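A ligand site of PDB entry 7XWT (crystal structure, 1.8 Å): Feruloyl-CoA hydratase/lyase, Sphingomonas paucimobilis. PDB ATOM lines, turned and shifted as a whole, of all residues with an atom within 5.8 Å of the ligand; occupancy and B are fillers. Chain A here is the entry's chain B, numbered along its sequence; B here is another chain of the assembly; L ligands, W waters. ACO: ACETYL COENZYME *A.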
ATOM      1  N   THR A  32      26.545 -33.309 -32.147  1.00  0.00           N
ATOM      2  CA  THR A  32      27.161 -33.669 -30.827  1.00  0.00           C
ATOM      3  C   THR A  32      26.872 -32.557 -29.813  1.00  0.00           C
ATOM      4  O   THR A  32      27.017 -32.813 -28.640  1.00  0.00           O
ATOM      5  CB  THR A  32      28.675 -33.940 -30.928  1.00  0.00           C
ATOM      6  OG1 THR A  32      29.314 -32.718 -31.270  1.00  0.00           O
ATOM      7  CG2 THR A  32      29.047 -34.984 -31.956  1.00  0.00           C
ATOM      8  N   LYS A  33      26.451 -31.385 -30.272  1.00  0.00           N
ATOM      9  CA  LYS A  33      25.949 -30.270 -29.429  1.00  0.00           C
ATOM     10  C   LYS A  33      24.423 -30.127 -29.508  1.00  0.00           C
ATOM     11  O   LYS A  33      23.891 -29.030 -29.169  1.00  0.00           O
ATOM     12  CB  LYS A  33      26.624 -28.987 -29.916  1.00  0.00           C
ATOM     13  CG  LYS A  33      28.119 -28.945 -29.661  1.00  0.00           C
ATOM     14  CD  LYS A  33      28.456 -28.923 -28.182  1.00  0.00           C
ATOM     15  CE  LYS A  33      29.929 -28.740 -27.878  1.00  0.00           C
ATOM     16  NZ  LYS A  33      30.141 -28.834 -26.417  1.00  0.00           N
ATOM     17  N   ARG A  34      23.731 -31.197 -29.921  1.00  0.00           N
ATOM     18  CA  ARG A  34      22.256 -31.230 -30.062  1.00  0.00           C
ATOM     19  C   ARG A  34      21.743 -30.032 -30.888  1.00  0.00           C
ATOM     20  O   ARG A  34      20.648 -29.589 -30.604  1.00  0.00           O
ATOM     21  CB  ARG A  34      21.672 -31.273 -28.643  1.00  0.00           C
ATOM     22  CG  ARG A  34      22.153 -32.444 -27.795  1.00  0.00           C
ATOM     23  CD  ARG A  34      21.735 -33.741 -28.449  1.00  0.00           C
ATOM     24  NE  ARG A  34      22.202 -34.915 -27.746  1.00  0.00           N
ATOM     25  CZ  ARG A  34      23.315 -35.602 -28.016  1.00  0.00           C
ATOM     26  NH1 ARG A  34      23.604 -36.665 -27.277  1.00  0.00           N
ATOM     27  NH2 ARG A  34      24.139 -35.243 -28.983  1.00  0.00           N
ATOM     28  N   ALA A  36      22.441 -26.978 -31.128  1.00  0.00           N
ATOM     29  CA  ALA A  36      22.270 -25.701 -30.411  1.00  0.00           C
ATOM     30  C   ALA A  36      22.633 -24.560 -31.343  1.00  0.00           C
ATOM     31  O   ALA A  36      23.569 -24.720 -32.163  1.00  0.00           O
ATOM     32  CB  ALA A  36      23.064 -25.696 -29.137  1.00  0.00           C
ATOM     33  N   PRO A  68      20.375 -36.842 -32.574  1.00  0.00           N
ATOM     34  CA  PRO A  68      19.129 -37.105 -31.857  1.00  0.00           C
ATOM     35  C   PRO A  68      18.275 -35.847 -31.605  1.00  0.00           C
ATOM     36  O   PRO A  68      17.122 -36.021 -31.374  1.00  0.00           O
ATOM     37  CB  PRO A  68      19.588 -37.737 -30.540  1.00  0.00           C
ATOM     38  CG  PRO A  68      21.014 -37.285 -30.350  1.00  0.00           C
ATOM     39  CD  PRO A  68      21.556 -36.916 -31.714  1.00  0.00           C
ATOM     40  N   ALA A  72      18.152 -27.996 -29.913  1.00  0.00           N
ATOM     41  CA  ALA A  72      18.000 -27.954 -28.441  1.00  0.00           C
ATOM     42  C   ALA A  72      18.075 -26.506 -27.980  1.00  0.00           C
ATOM     43  O   ALA A  72      18.436 -26.309 -26.837  1.00  0.00           O
ATOM     44  CB  ALA A  72      19.018 -28.833 -27.741  1.00  0.00           C
ATOM     45  N   GLY A  73      17.798 -25.550 -28.857  1.00  0.00           N
ATOM     46  CA  GLY A  73      17.701 -24.142 -28.440  1.00  0.00           C
ATOM     47  C   GLY A  73      18.933 -23.357 -28.736  1.00  0.00           C
ATOM     48  O   GLY A  73      19.701 -23.759 -29.584  1.00  0.00           O
ATOM     49  N   MET A  74      19.095 -22.215 -28.076  1.00  0.00           N
ATOM     50  CA  MET A  74      20.305 -21.407 -28.184  1.00  0.00           C
ATOM     51  C   MET A  74      21.461 -22.142 -27.469  1.00  0.00           C
ATOM     52  O   MET A  74      21.232 -22.979 -26.552  1.00  0.00           O
ATOM     53  CB  MET A  74      20.075 -20.031 -27.572  1.00  0.00           C
ATOM     54  CG  MET A  74      18.786 -19.354 -28.058  1.00  0.00           C
ATOM     55  SD  MET A  74      18.416 -19.514 -29.831  1.00  0.00           S
ATOM     56  CE  MET A  74      19.598 -18.378 -30.548  1.00  0.00           C
ATOM     57  N   ASP A  75      22.663 -21.901 -27.966  1.00  0.00           N
ATOM     58  CA  ASP A  75      23.909 -22.405 -27.356  1.00  0.00           C
ATOM     59  C   ASP A  75      24.199 -21.595 -26.080  1.00  0.00           C
ATOM     60  O   ASP A  75      24.650 -20.415 -26.214  1.00  0.00           O
ATOM     61  CB  ASP A  75      25.041 -22.392 -28.389  1.00  0.00           C
ATOM     62  CG  ASP A  75      26.264 -23.180 -27.900  1.00  0.00           C
ATOM     63  OD1 ASP A  75      26.610 -23.037 -26.712  1.00  0.00           O
ATOM     64  OD2 ASP A  75      26.813 -23.964 -28.717  1.00  0.00           O
ATOM     65  N   LEU A  76      24.010 -22.230 -24.916  1.00  0.00           N
ATOM     66  CA  LEU A  76      24.207 -21.583 -23.583  1.00  0.00           C
ATOM     67  C   LEU A  76      25.649 -21.083 -23.499  1.00  0.00           C
ATOM     68  O   LEU A  76      25.845 -19.987 -22.940  1.00  0.00           O
ATOM     69  CB  LEU A  76      23.898 -22.536 -22.430  1.00  0.00           C
ATOM     70  CG  LEU A  76      22.432 -22.924 -22.155  1.00  0.00           C
ATOM     71  CD1 LEU A  76      22.075 -22.742 -20.696  1.00  0.00           C
ATOM     72  CD2 LEU A  76      21.418 -22.185 -23.020  1.00  0.00           C
ATOM     73  N   LYS A  77      26.615 -21.777 -24.131  1.00  0.00           N
ATOM     74  CA  LYS A  77      28.040 -21.363 -24.120  1.00  0.00           C
ATOM     75  C   LYS A  77      28.290 -20.243 -25.121  1.00  0.00           C
ATOM     76  O   LYS A  77      28.723 -19.165 -24.693  1.00  0.00           O
ATOM     77  CB  LYS A  77      28.941 -22.567 -24.371  1.00  0.00           C
ATOM     78  CG  LYS A  77      30.404 -22.377 -24.008  1.00  0.00           C
ATOM     79  CD  LYS A  77      31.262 -23.600 -24.315  1.00  0.00           C
ATOM     80  CE  LYS A  77      32.729 -23.228 -24.445  1.00  0.00           C
ATOM     81  NZ  LYS A  77      33.553 -24.412 -24.814  1.00  0.00           N
ATOM     82  N   PHE A  80      24.981 -17.291 -25.401  1.00  0.00           N
ATOM     83  CA  PHE A  80      24.778 -16.561 -24.119  1.00  0.00           C
ATOM     84  C   PHE A  80      26.129 -16.232 -23.455  1.00  0.00           C
ATOM     85  O   PHE A  80      26.513 -15.043 -23.499  1.00  0.00           O
ATOM     86  CB  PHE A  80      23.812 -17.312 -23.208  1.00  0.00           C
ATOM     87  CG  PHE A  80      22.377 -17.217 -23.634  1.00  0.00           C
ATOM     88  CD1 PHE A  80      21.725 -15.982 -23.702  1.00  0.00           C
ATOM     89  CD2 PHE A  80      21.673 -18.359 -23.979  1.00  0.00           C
ATOM     90  CE1 PHE A  80      20.379 -15.905 -24.069  1.00  0.00           C
ATOM     91  CE2 PHE A  80      20.341 -18.276 -24.365  1.00  0.00           C
ATOM     92  CZ  PHE A  80      19.691 -17.057 -24.399  1.00  0.00           C
ATOM     93  N   TRP A 119      14.543 -33.722 -30.155  1.00  0.00           N
ATOM     94  CA  TRP A 119      14.493 -32.617 -29.159  1.00  0.00           C
ATOM     95  C   TRP A 119      14.210 -31.320 -29.887  1.00  0.00           C
ATOM     96  O   TRP A 119      14.892 -31.042 -30.858  1.00  0.00           O
ATOM     97  CB  TRP A 119      15.815 -32.506 -28.380  1.00  0.00           C
ATOM     98  CG  TRP A 119      16.276 -33.762 -27.699  1.00  0.00           C
ATOM     99  CD1 TRP A 119      17.374 -34.505 -28.036  1.00  0.00           C
ATOM    100  CD2 TRP A 119      15.683 -34.392 -26.565  1.00  0.00           C
ATOM    101  NE1 TRP A 119      17.479 -35.582 -27.194  1.00  0.00           N
ATOM    102  CE2 TRP A 119      16.470 -35.534 -26.281  1.00  0.00           C
ATOM    103  CE3 TRP A 119      14.587 -34.118 -25.748  1.00  0.00           C
ATOM    104  CZ2 TRP A 119      16.180 -36.399 -25.228  1.00  0.00           C
ATOM    105  CZ3 TRP A 119      14.292 -34.973 -24.707  1.00  0.00           C
ATOM    106  CH2 TRP A 119      15.085 -36.098 -24.445  1.00  0.00           C
ATOM    107  N   PHE A 121      13.658 -27.433 -28.241  1.00  0.00           N
ATOM    108  CA  PHE A 121      13.653 -26.692 -26.967  1.00  0.00           C
ATOM    109  C   PHE A 121      13.822 -25.196 -27.190  1.00  0.00           C
ATOM    110  O   PHE A 121      14.645 -24.779 -28.001  1.00  0.00           O
ATOM    111  CB  PHE A 121      14.753 -27.148 -25.990  1.00  0.00           C
ATOM    112  CG  PHE A 121      14.483 -28.524 -25.430  1.00  0.00           C
ATOM    113  CD1 PHE A 121      13.354 -28.758 -24.666  1.00  0.00           C
ATOM    114  CD2 PHE A 121      15.350 -29.568 -25.667  1.00  0.00           C
ATOM    115  CE1 PHE A 121      13.099 -30.019 -24.160  1.00  0.00           C
ATOM    116  CE2 PHE A 121      15.076 -30.849 -25.182  1.00  0.00           C
ATOM    117  CZ  PHE A 121      13.969 -31.055 -24.407  1.00  0.00           C
ATOM    118  N   GLY A 122      13.026 -24.455 -26.452  1.00  0.00           N
ATOM    119  CA  GLY A 122      13.308 -23.021 -26.229  1.00  0.00           C
ATOM    120  C   GLY A 122      13.383 -22.249 -27.512  1.00  0.00           C
ATOM    121  O   GLY A 122      12.365 -22.172 -28.201  1.00  0.00           O
ATOM    122  N   GLY A 123      14.526 -21.619 -27.763  1.00  0.00           N
ATOM    123  CA  GLY A 123      14.823 -20.755 -28.916  1.00  0.00           C
ATOM    124  C   GLY A 123      14.779 -21.496 -30.251  1.00  0.00           C
ATOM    125  O   GLY A 123      14.860 -20.840 -31.263  1.00  0.00           O
ATOM    126  N   ALA A 124      14.570 -22.815 -30.241  1.00  0.00           N
ATOM    127  CA  ALA A 124      14.141 -23.579 -31.456  1.00  0.00           C
ATOM    128  C   ALA A 124      12.680 -23.278 -31.882  1.00  0.00           C
ATOM    129  O   ALA A 124      12.324 -23.630 -33.045  1.00  0.00           O
ATOM    130  CB  ALA A 124      14.266 -25.076 -31.221  1.00  0.00           C
ATOM    131  N   SER A 145      11.835 -24.998 -22.068  1.00  0.00           N
ATOM    132  CA  SER A 145      12.712 -25.408 -20.962  1.00  0.00           C
ATOM    133  C   SER A 145      13.285 -24.152 -20.287  1.00  0.00           C
ATOM    134  O   SER A 145      13.945 -24.274 -19.256  1.00  0.00           O
ATOM    135  CB  SER A 145      13.794 -26.304 -21.528  1.00  0.00           C
ATOM    136  OG  SER A 145      14.357 -25.736 -22.710  1.00  0.00           O
ATOM    137  N   GLU A 146      13.049 -22.967 -20.848  1.00  0.00           N
ATOM    138  CA  GLU A 146      13.592 -21.692 -20.324  1.00  0.00           C
ATOM    139  C   GLU A 146      13.338 -21.579 -18.807  1.00  0.00           C
ATOM    140  O   GLU A 146      14.289 -21.237 -18.082  1.00  0.00           O
ATOM    141  CB  GLU A 146      13.041 -20.515 -21.124  1.00  0.00           C
ATOM    142  CG  GLU A 146      13.543 -20.444 -22.580  1.00  0.00           C
ATOM    143  CD  GLU A 146      12.573 -20.961 -23.645  1.00  0.00           C
ATOM    144  OE1 GLU A 146      12.510 -20.397 -24.772  1.00  0.00           O
ATOM    145  OE2 GLU A 146      11.860 -21.945 -23.356  1.00  0.00           O
ATOM    146  N   TRP A 149      15.841 -23.166 -16.469  1.00  0.00           N
ATOM    147  CA  TRP A 149      17.180 -22.579 -16.270  1.00  0.00           C
ATOM    148  C   TRP A 149      17.035 -21.090 -15.923  1.00  0.00           C
ATOM    149  O   TRP A 149      18.019 -20.419 -16.012  1.00  0.00           O
ATOM    150  CB  TRP A 149      18.149 -22.910 -17.429  1.00  0.00           C
ATOM    151  CG  TRP A 149      18.057 -22.221 -18.751  1.00  0.00           C
ATOM    152  CD1 TRP A 149      17.303 -22.587 -19.828  1.00  0.00           C
ATOM    153  CD2 TRP A 149      18.849 -21.103 -19.207  1.00  0.00           C
ATOM    154  NE1 TRP A 149      17.538 -21.767 -20.895  1.00  0.00           N
ATOM    155  CE2 TRP A 149      18.490 -20.843 -20.541  1.00  0.00           C
ATOM    156  CE3 TRP A 149      19.832 -20.291 -18.608  1.00  0.00           C
ATOM    157  CZ2 TRP A 149      19.060 -19.793 -21.282  1.00  0.00           C
ATOM    158  CZ3 TRP A 149      20.408 -19.272 -19.344  1.00  0.00           C
ATOM    159  CH2 TRP A 149      20.024 -19.038 -20.669  1.00  0.00           C
ATOM    160  N   ILE A 151      15.214 -18.440 -16.939  1.00  0.00           N
ATOM    161  CA  ILE A 151      14.923 -17.308 -17.893  1.00  0.00           C
ATOM    162  C   ILE A 151      13.476 -17.434 -18.405  1.00  0.00           C
ATOM    163  O   ILE A 151      12.871 -18.521 -18.371  1.00  0.00           O
ATOM    164  CB  ILE A 151      15.912 -17.226 -19.050  1.00  0.00           C
ATOM    165  CG1 ILE A 151      15.879 -18.490 -19.927  1.00  0.00           C
ATOM    166  CG2 ILE A 151      17.297 -16.916 -18.522  1.00  0.00           C
ATOM    167  CD1 ILE A 151      16.171 -18.226 -21.394  1.00  0.00           C
ATOM    168  N   PHE B 264      24.610 -26.535 -15.674  1.00  0.00           N
ATOM    169  CA  PHE B 264      24.427 -27.251 -16.965  1.00  0.00           C
ATOM    170  C   PHE B 264      25.775 -27.361 -17.708  1.00  0.00           C
ATOM    171  O   PHE B 264      26.097 -28.479 -18.143  1.00  0.00           O
ATOM    172  CB  PHE B 264      23.371 -26.581 -17.869  1.00  0.00           C
ATOM    173  CG  PHE B 264      23.273 -27.225 -19.236  1.00  0.00           C
ATOM    174  CD1 PHE B 264      22.852 -28.548 -19.354  1.00  0.00           C
ATOM    175  CD2 PHE B 264      23.649 -26.534 -20.374  1.00  0.00           C
ATOM    176  CE1 PHE B 264      22.788 -29.155 -20.607  1.00  0.00           C
ATOM    177  CE2 PHE B 264      23.575 -27.140 -21.629  1.00  0.00           C
ATOM    178  CZ  PHE B 264      23.136 -28.439 -21.744  1.00  0.00           C
ATOM    179  N   LEU B 265      26.463 -26.236 -17.937  1.00  0.00           N
ATOM    180  CA  LEU B 265      27.707 -26.135 -18.746  1.00  0.00           C
ATOM    181  C   LEU B 265      28.937 -26.692 -17.979  1.00  0.00           C
ATOM    182  O   LEU B 265      29.703 -27.486 -18.593  1.00  0.00           O
ATOM    183  CB  LEU B 265      27.960 -24.675 -19.105  1.00  0.00           C
ATOM    184  CG  LEU B 265      26.991 -24.049 -20.121  1.00  0.00           C
ATOM    185  CD1 LEU B 265      27.373 -22.612 -20.423  1.00  0.00           C
ATOM    186  CD2 LEU B 265      26.951 -24.857 -21.416  1.00  0.00           C
ATOM    187  N   LYS B 268      27.534 -30.012 -15.015  1.00  0.00           N
ATOM    188  CA  LYS B 268      26.703 -31.048 -15.702  1.00  0.00           C
ATOM    189  C   LYS B 268      25.884 -31.872 -14.695  1.00  0.00           C
ATOM    190  O   LYS B 268      25.846 -33.109 -14.829  1.00  0.00           O
ATOM    191  CB  LYS B 268      27.547 -32.028 -16.524  1.00  0.00           C
ATOM    192  CG  LYS B 268      28.858 -31.483 -17.071  1.00  0.00           C
ATOM    193  CD  LYS B 268      28.715 -30.480 -18.187  1.00  0.00           C
ATOM    194  CE  LYS B 268      29.925 -30.454 -19.084  1.00  0.00           C
ATOM    195  NZ  LYS B 268      29.916 -31.605 -20.012  1.00  0.00           N
ATOM    196  N   LYS B 271      20.004 -31.166 -16.854  1.00  0.00           N
ATOM    197  CA  LYS B 271      19.656 -30.855 -18.264  1.00  0.00           C
ATOM    198  C   LYS B 271      18.331 -30.085 -18.287  1.00  0.00           C
ATOM    199  O   LYS B 271      17.274 -30.627 -17.941  1.00  0.00           O
ATOM    200  CB  LYS B 271      19.557 -32.186 -19.001  1.00  0.00           C
ATOM    201  CG  LYS B 271      20.845 -32.991 -19.082  1.00  0.00           C
ATOM    202  CD  LYS B 271      20.600 -34.479 -19.374  1.00  0.00           C
ATOM    203  CE  LYS B 271      21.879 -35.304 -19.362  1.00  0.00           C
ATOM    204  NZ  LYS B 271      21.691 -36.623 -20.003  1.00  0.00           N
ATOM    205  N   PRO B 272      18.322 -28.765 -18.602  1.00  0.00           N
ATOM    206  CA  PRO B 272      17.076 -27.994 -18.498  1.00  0.00           C
ATOM    207  C   PRO B 272      15.922 -28.524 -19.358  1.00  0.00           C
ATOM    208  O   PRO B 272      14.795 -28.340 -18.974  1.00  0.00           O
ATOM    209  CB  PRO B 272      17.442 -26.541 -18.867  1.00  0.00           C
ATOM    210  CG  PRO B 272      18.957 -26.522 -19.106  1.00  0.00           C
ATOM    211  CD  PRO B 272      19.485 -27.933 -18.935  1.00  0.00           C
ATOM    212  N   GLY B 273      16.210 -29.170 -20.493  1.00  0.00           N
ATOM    213  CA  GLY B 273      15.178 -29.854 -21.291  1.00  0.00           C
ATOM    214  C   GLY B 273      14.439 -30.912 -20.476  1.00  0.00           C
ATOM    215  O   GLY B 273      13.339 -31.313 -20.892  1.00  0.00           O
ATOM    216  N   LEU B 274      15.021 -31.381 -19.373  1.00  0.00           N
ATOM    217  CA  LEU B 274      14.476 -32.578 -18.649  1.00  0.00           C
ATOM    218  C   LEU B 274      14.084 -32.259 -17.193  1.00  0.00           C
ATOM    219  O   LEU B 274      13.437 -33.116 -16.571  1.00  0.00           O
ATOM    220  CB  LEU B 274      15.533 -33.680 -18.682  1.00  0.00           C
ATOM    221  CG  LEU B 274      15.815 -34.270 -20.071  1.00  0.00           C
ATOM    222  CD1 LEU B 274      16.940 -35.298 -19.978  1.00  0.00           C
ATOM    223  CD2 LEU B 274      14.562 -34.904 -20.699  1.00  0.00           C
HETATM  224  N1A ACO L   1      23.587 -25.223 -25.485  1.00  0.00           N
HETATM  225  C2A ACO L   1      24.841 -25.674 -25.526  1.00  0.00           C
HETATM  226  N3A ACO L   1      25.286 -26.926 -25.513  1.00  0.00           N
HETATM  227  C4A ACO L   1      24.285 -27.791 -25.463  1.00  0.00           C
HETATM  228  C5A ACO L   1      22.954 -27.493 -25.437  1.00  0.00           C
HETATM  229  C6A ACO L   1      22.584 -26.130 -25.451  1.00  0.00           C
HETATM  230  N6A ACO L   1      21.327 -25.715 -25.468  1.00  0.00           N
HETATM  231  N7A ACO L   1      22.210 -28.658 -25.376  1.00  0.00           N
HETATM  232  C8A ACO L   1      23.094 -29.620 -25.375  1.00  0.00           C
HETATM  233  N9A ACO L   1      24.367 -29.164 -25.457  1.00  0.00           N
HETATM  234  C1B ACO L   1      25.582 -29.977 -25.427  1.00  0.00           C
HETATM  235  C2B ACO L   1      25.919 -30.481 -24.025  1.00  0.00           C
HETATM  236  O2B ACO L   1      26.529 -29.493 -23.237  1.00  0.00           O
HETATM  237  C3B ACO L   1      26.863 -31.628 -24.358  1.00  0.00           C
HETATM  238  O3B ACO L   1      28.129 -31.049 -24.641  1.00  0.00           O
HETATM  239  P3B ACO L   1      29.467 -31.885 -24.249  1.00  0.00           P
HETATM  240  O7A ACO L   1      29.189 -33.349 -24.458  1.00  0.00           O
HETATM  241  O8A ACO L   1      29.811 -31.565 -22.829  1.00  0.00           O
HETATM  242  O9A ACO L   1      30.437 -31.316 -25.248  1.00  0.00           O
HETATM  243  C4B ACO L   1      26.194 -32.228 -25.604  1.00  0.00           C
HETATM  244  O4B ACO L   1      25.380 -31.162 -26.170  1.00  0.00           O
HETATM  245  C5B ACO L   1      25.316 -33.435 -25.347  1.00  0.00           C
HETATM  246  O5B ACO L   1      24.290 -33.006 -24.414  1.00  0.00           O
HETATM  247  P1A ACO L   1      23.654 -33.938 -23.311  1.00  0.00           P
HETATM  248  O1A ACO L   1      24.591 -35.002 -22.847  1.00  0.00           O
HETATM  249  O2A ACO L   1      23.036 -33.099 -22.257  1.00  0.00           O
HETATM  250  O3A ACO L   1      22.610 -34.696 -24.255  1.00  0.00           O
HETATM  251  P2A ACO L   1      21.446 -35.772 -24.023  1.00  0.00           P
HETATM  252  O4A ACO L   1      21.579 -36.501 -22.729  1.00  0.00           O
HETATM  253  O5A ACO L   1      21.059 -36.505 -25.275  1.00  0.00           O
HETATM  254  O6A ACO L   1      20.192 -34.821 -23.760  1.00  0.00           O
HETATM  255  CBP ACO L   1      19.417 -32.670 -23.598  1.00  0.00           C
HETATM  256  CCP ACO L   1      19.951 -33.683 -24.592  1.00  0.00           C
HETATM  257  CDP ACO L   1      17.917 -32.953 -23.342  1.00  0.00           C
HETATM  258  CEP ACO L   1      20.212 -32.784 -22.299  1.00  0.00           C
HETATM  259  CAP ACO L   1      19.624 -31.266 -24.080  1.00  0.00           C
HETATM  260  OAP ACO L   1      18.661 -31.236 -25.142  1.00  0.00           O
HETATM  261  C9P ACO L   1      19.451 -30.195 -22.999  1.00  0.00           C
HETATM  262  O9P ACO L   1      18.775 -30.346 -21.972  1.00  0.00           O
HETATM  263  N8P ACO L   1      20.105 -29.084 -23.222  1.00  0.00           N
HETATM  264  C7P ACO L   1      19.510 -27.772 -23.055  1.00  0.00           C
HETATM  265  C6P ACO L   1      18.165 -27.736 -23.723  1.00  0.00           C
HETATM  266  C5P ACO L   1      17.329 -26.816 -22.872  1.00  0.00           C
HETATM  267  O5P ACO L   1      16.760 -27.208 -21.867  1.00  0.00           O
HETATM  268  N4P ACO L   1      17.242 -25.562 -23.253  1.00  0.00           N
HETATM  269  C3P ACO L   1      17.146 -25.141 -24.623  1.00  0.00           C
HETATM  270  C2P ACO L   1      18.008 -23.955 -24.809  1.00  0.00           C
HETATM  271  S1P ACO L   1      17.146 -22.632 -23.932  1.00  0.00           S
HETATM  272  C   ACO L   1      17.275 -21.436 -25.056  1.00  0.00           C
HETATM  273  O   ACO L   1      16.987 -21.634 -26.206  1.00  0.00           O
HETATM  274  CH3 ACO L   1      17.793 -20.236 -24.506  1.00  0.00           C
HETATM  275  O   HOH W   1      26.509 -29.673 -20.772  1.00  0.00           O
HETATM  276  O   HOH W   2      25.182 -37.391 -23.706  1.00  0.00           O
HETATM  277  O   HOH W   3      28.066 -26.728 -25.278  1.00  0.00           O
HETATM  278  O   HOH W   4      28.326 -34.659 -27.151  1.00  0.00           O
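An oxygen (O9A) of the ligand is in salt-bridge range of the side-chain amino group (NZ) of Lys 33, at 2.8 Å. An oxygen (O5P) of the ligand is in hydrogen-bond range of the backbone NH (N) of Gly 273 of chain B (2.5 Å). The side-chain amino group (NZ) of Lys 271 of chain B is in salt-bridge range of an oxygen (O4A) of the ligand, 2.7 Å away. The side-chain hydroxyl of Ser 145 lies within hydrogen-bond range of a nitrogen (N4P) of the ligand, at 2.9 Å. An oxygen (O5A) of the ligand lies within salt-bridge range of the guanidinium group (NE) of Arg 34 (3.2 Å). N6A of the ligand sits at hydrogen-bond distance from O of Met 74 (2.9 Å). The backbone NH (N) of Gly 123 lies within hydrogen-bond range of an oxygen (O) of the ligand (2.9 Å). The backbone NH of Leu 76 is in hydrogen-bond range of a nitrogen (N1A) of the ligand, at 3.1 Å. The backbone NH (N) of Met 74 sits at hydrogen-bond distance from an oxygen (O) of the ligand, at 2.9 Å. NE1 of Trp 149 sits close to S1P of the ligand, at 3.2 Å. O of Ala 72 sits close to N6A of the ligand (3.3 Å). NZ of Lys 268 of chain B lies within salt-bridge range of O8A of the ligand (2.8 Å).
N of Phe 80 lies within hydrogen-bond range of O of Asp 75 (3.2 Å). The backbone carbonyl oxygen of Arg 34 is in hydrogen-bond range of the backbone NH of Ala 72 (3.0 Å). OD1 of Asp 75 is in hydrogen-bond range of N of Lys 77 (2.9 Å). The backbone NH of Gly 73 sits close to the backbone carbonyl oxygen of Phe 121 (3.4 Å).
An oxygen (O4B) of the ligand sits close to the backbone carbonyl oxygen (O) of Thr 32. Merely in contact with the ligand: Pro 272 of chain B (3.0 Å), Phe 80 (3.2 Å), Asp 75 (3.4 Å), Phe 121 (3.4 Å), Phe 264 of chain B (3.4 Å), Gly 73 (3.4 Å), Ala 36 (3.7 Å) and Gly 122 (3.9 Å). The nearest printed residue that does not touch the ligand is Ile 151 (4.04 Å).
Water W1 bridges an oxygen (O2B) of the ligand (2.5 Å) and the backbone carbonyl oxygen (O) of Phe 264 of chain B (2.9 Å). Water W3 lies within hydrogen-bond range of a nitrogen (N3A) of the ligand (2.8 Å) and the side-chain amino group (NZ) of Lys 33 (3.2 Å). Water W4 lies within hydrogen-bond range of the backbone carbonyl oxygen (O) of Thr 32 (2.7 Å) and an oxygen (O7A) of the ligand (3.1 Å).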
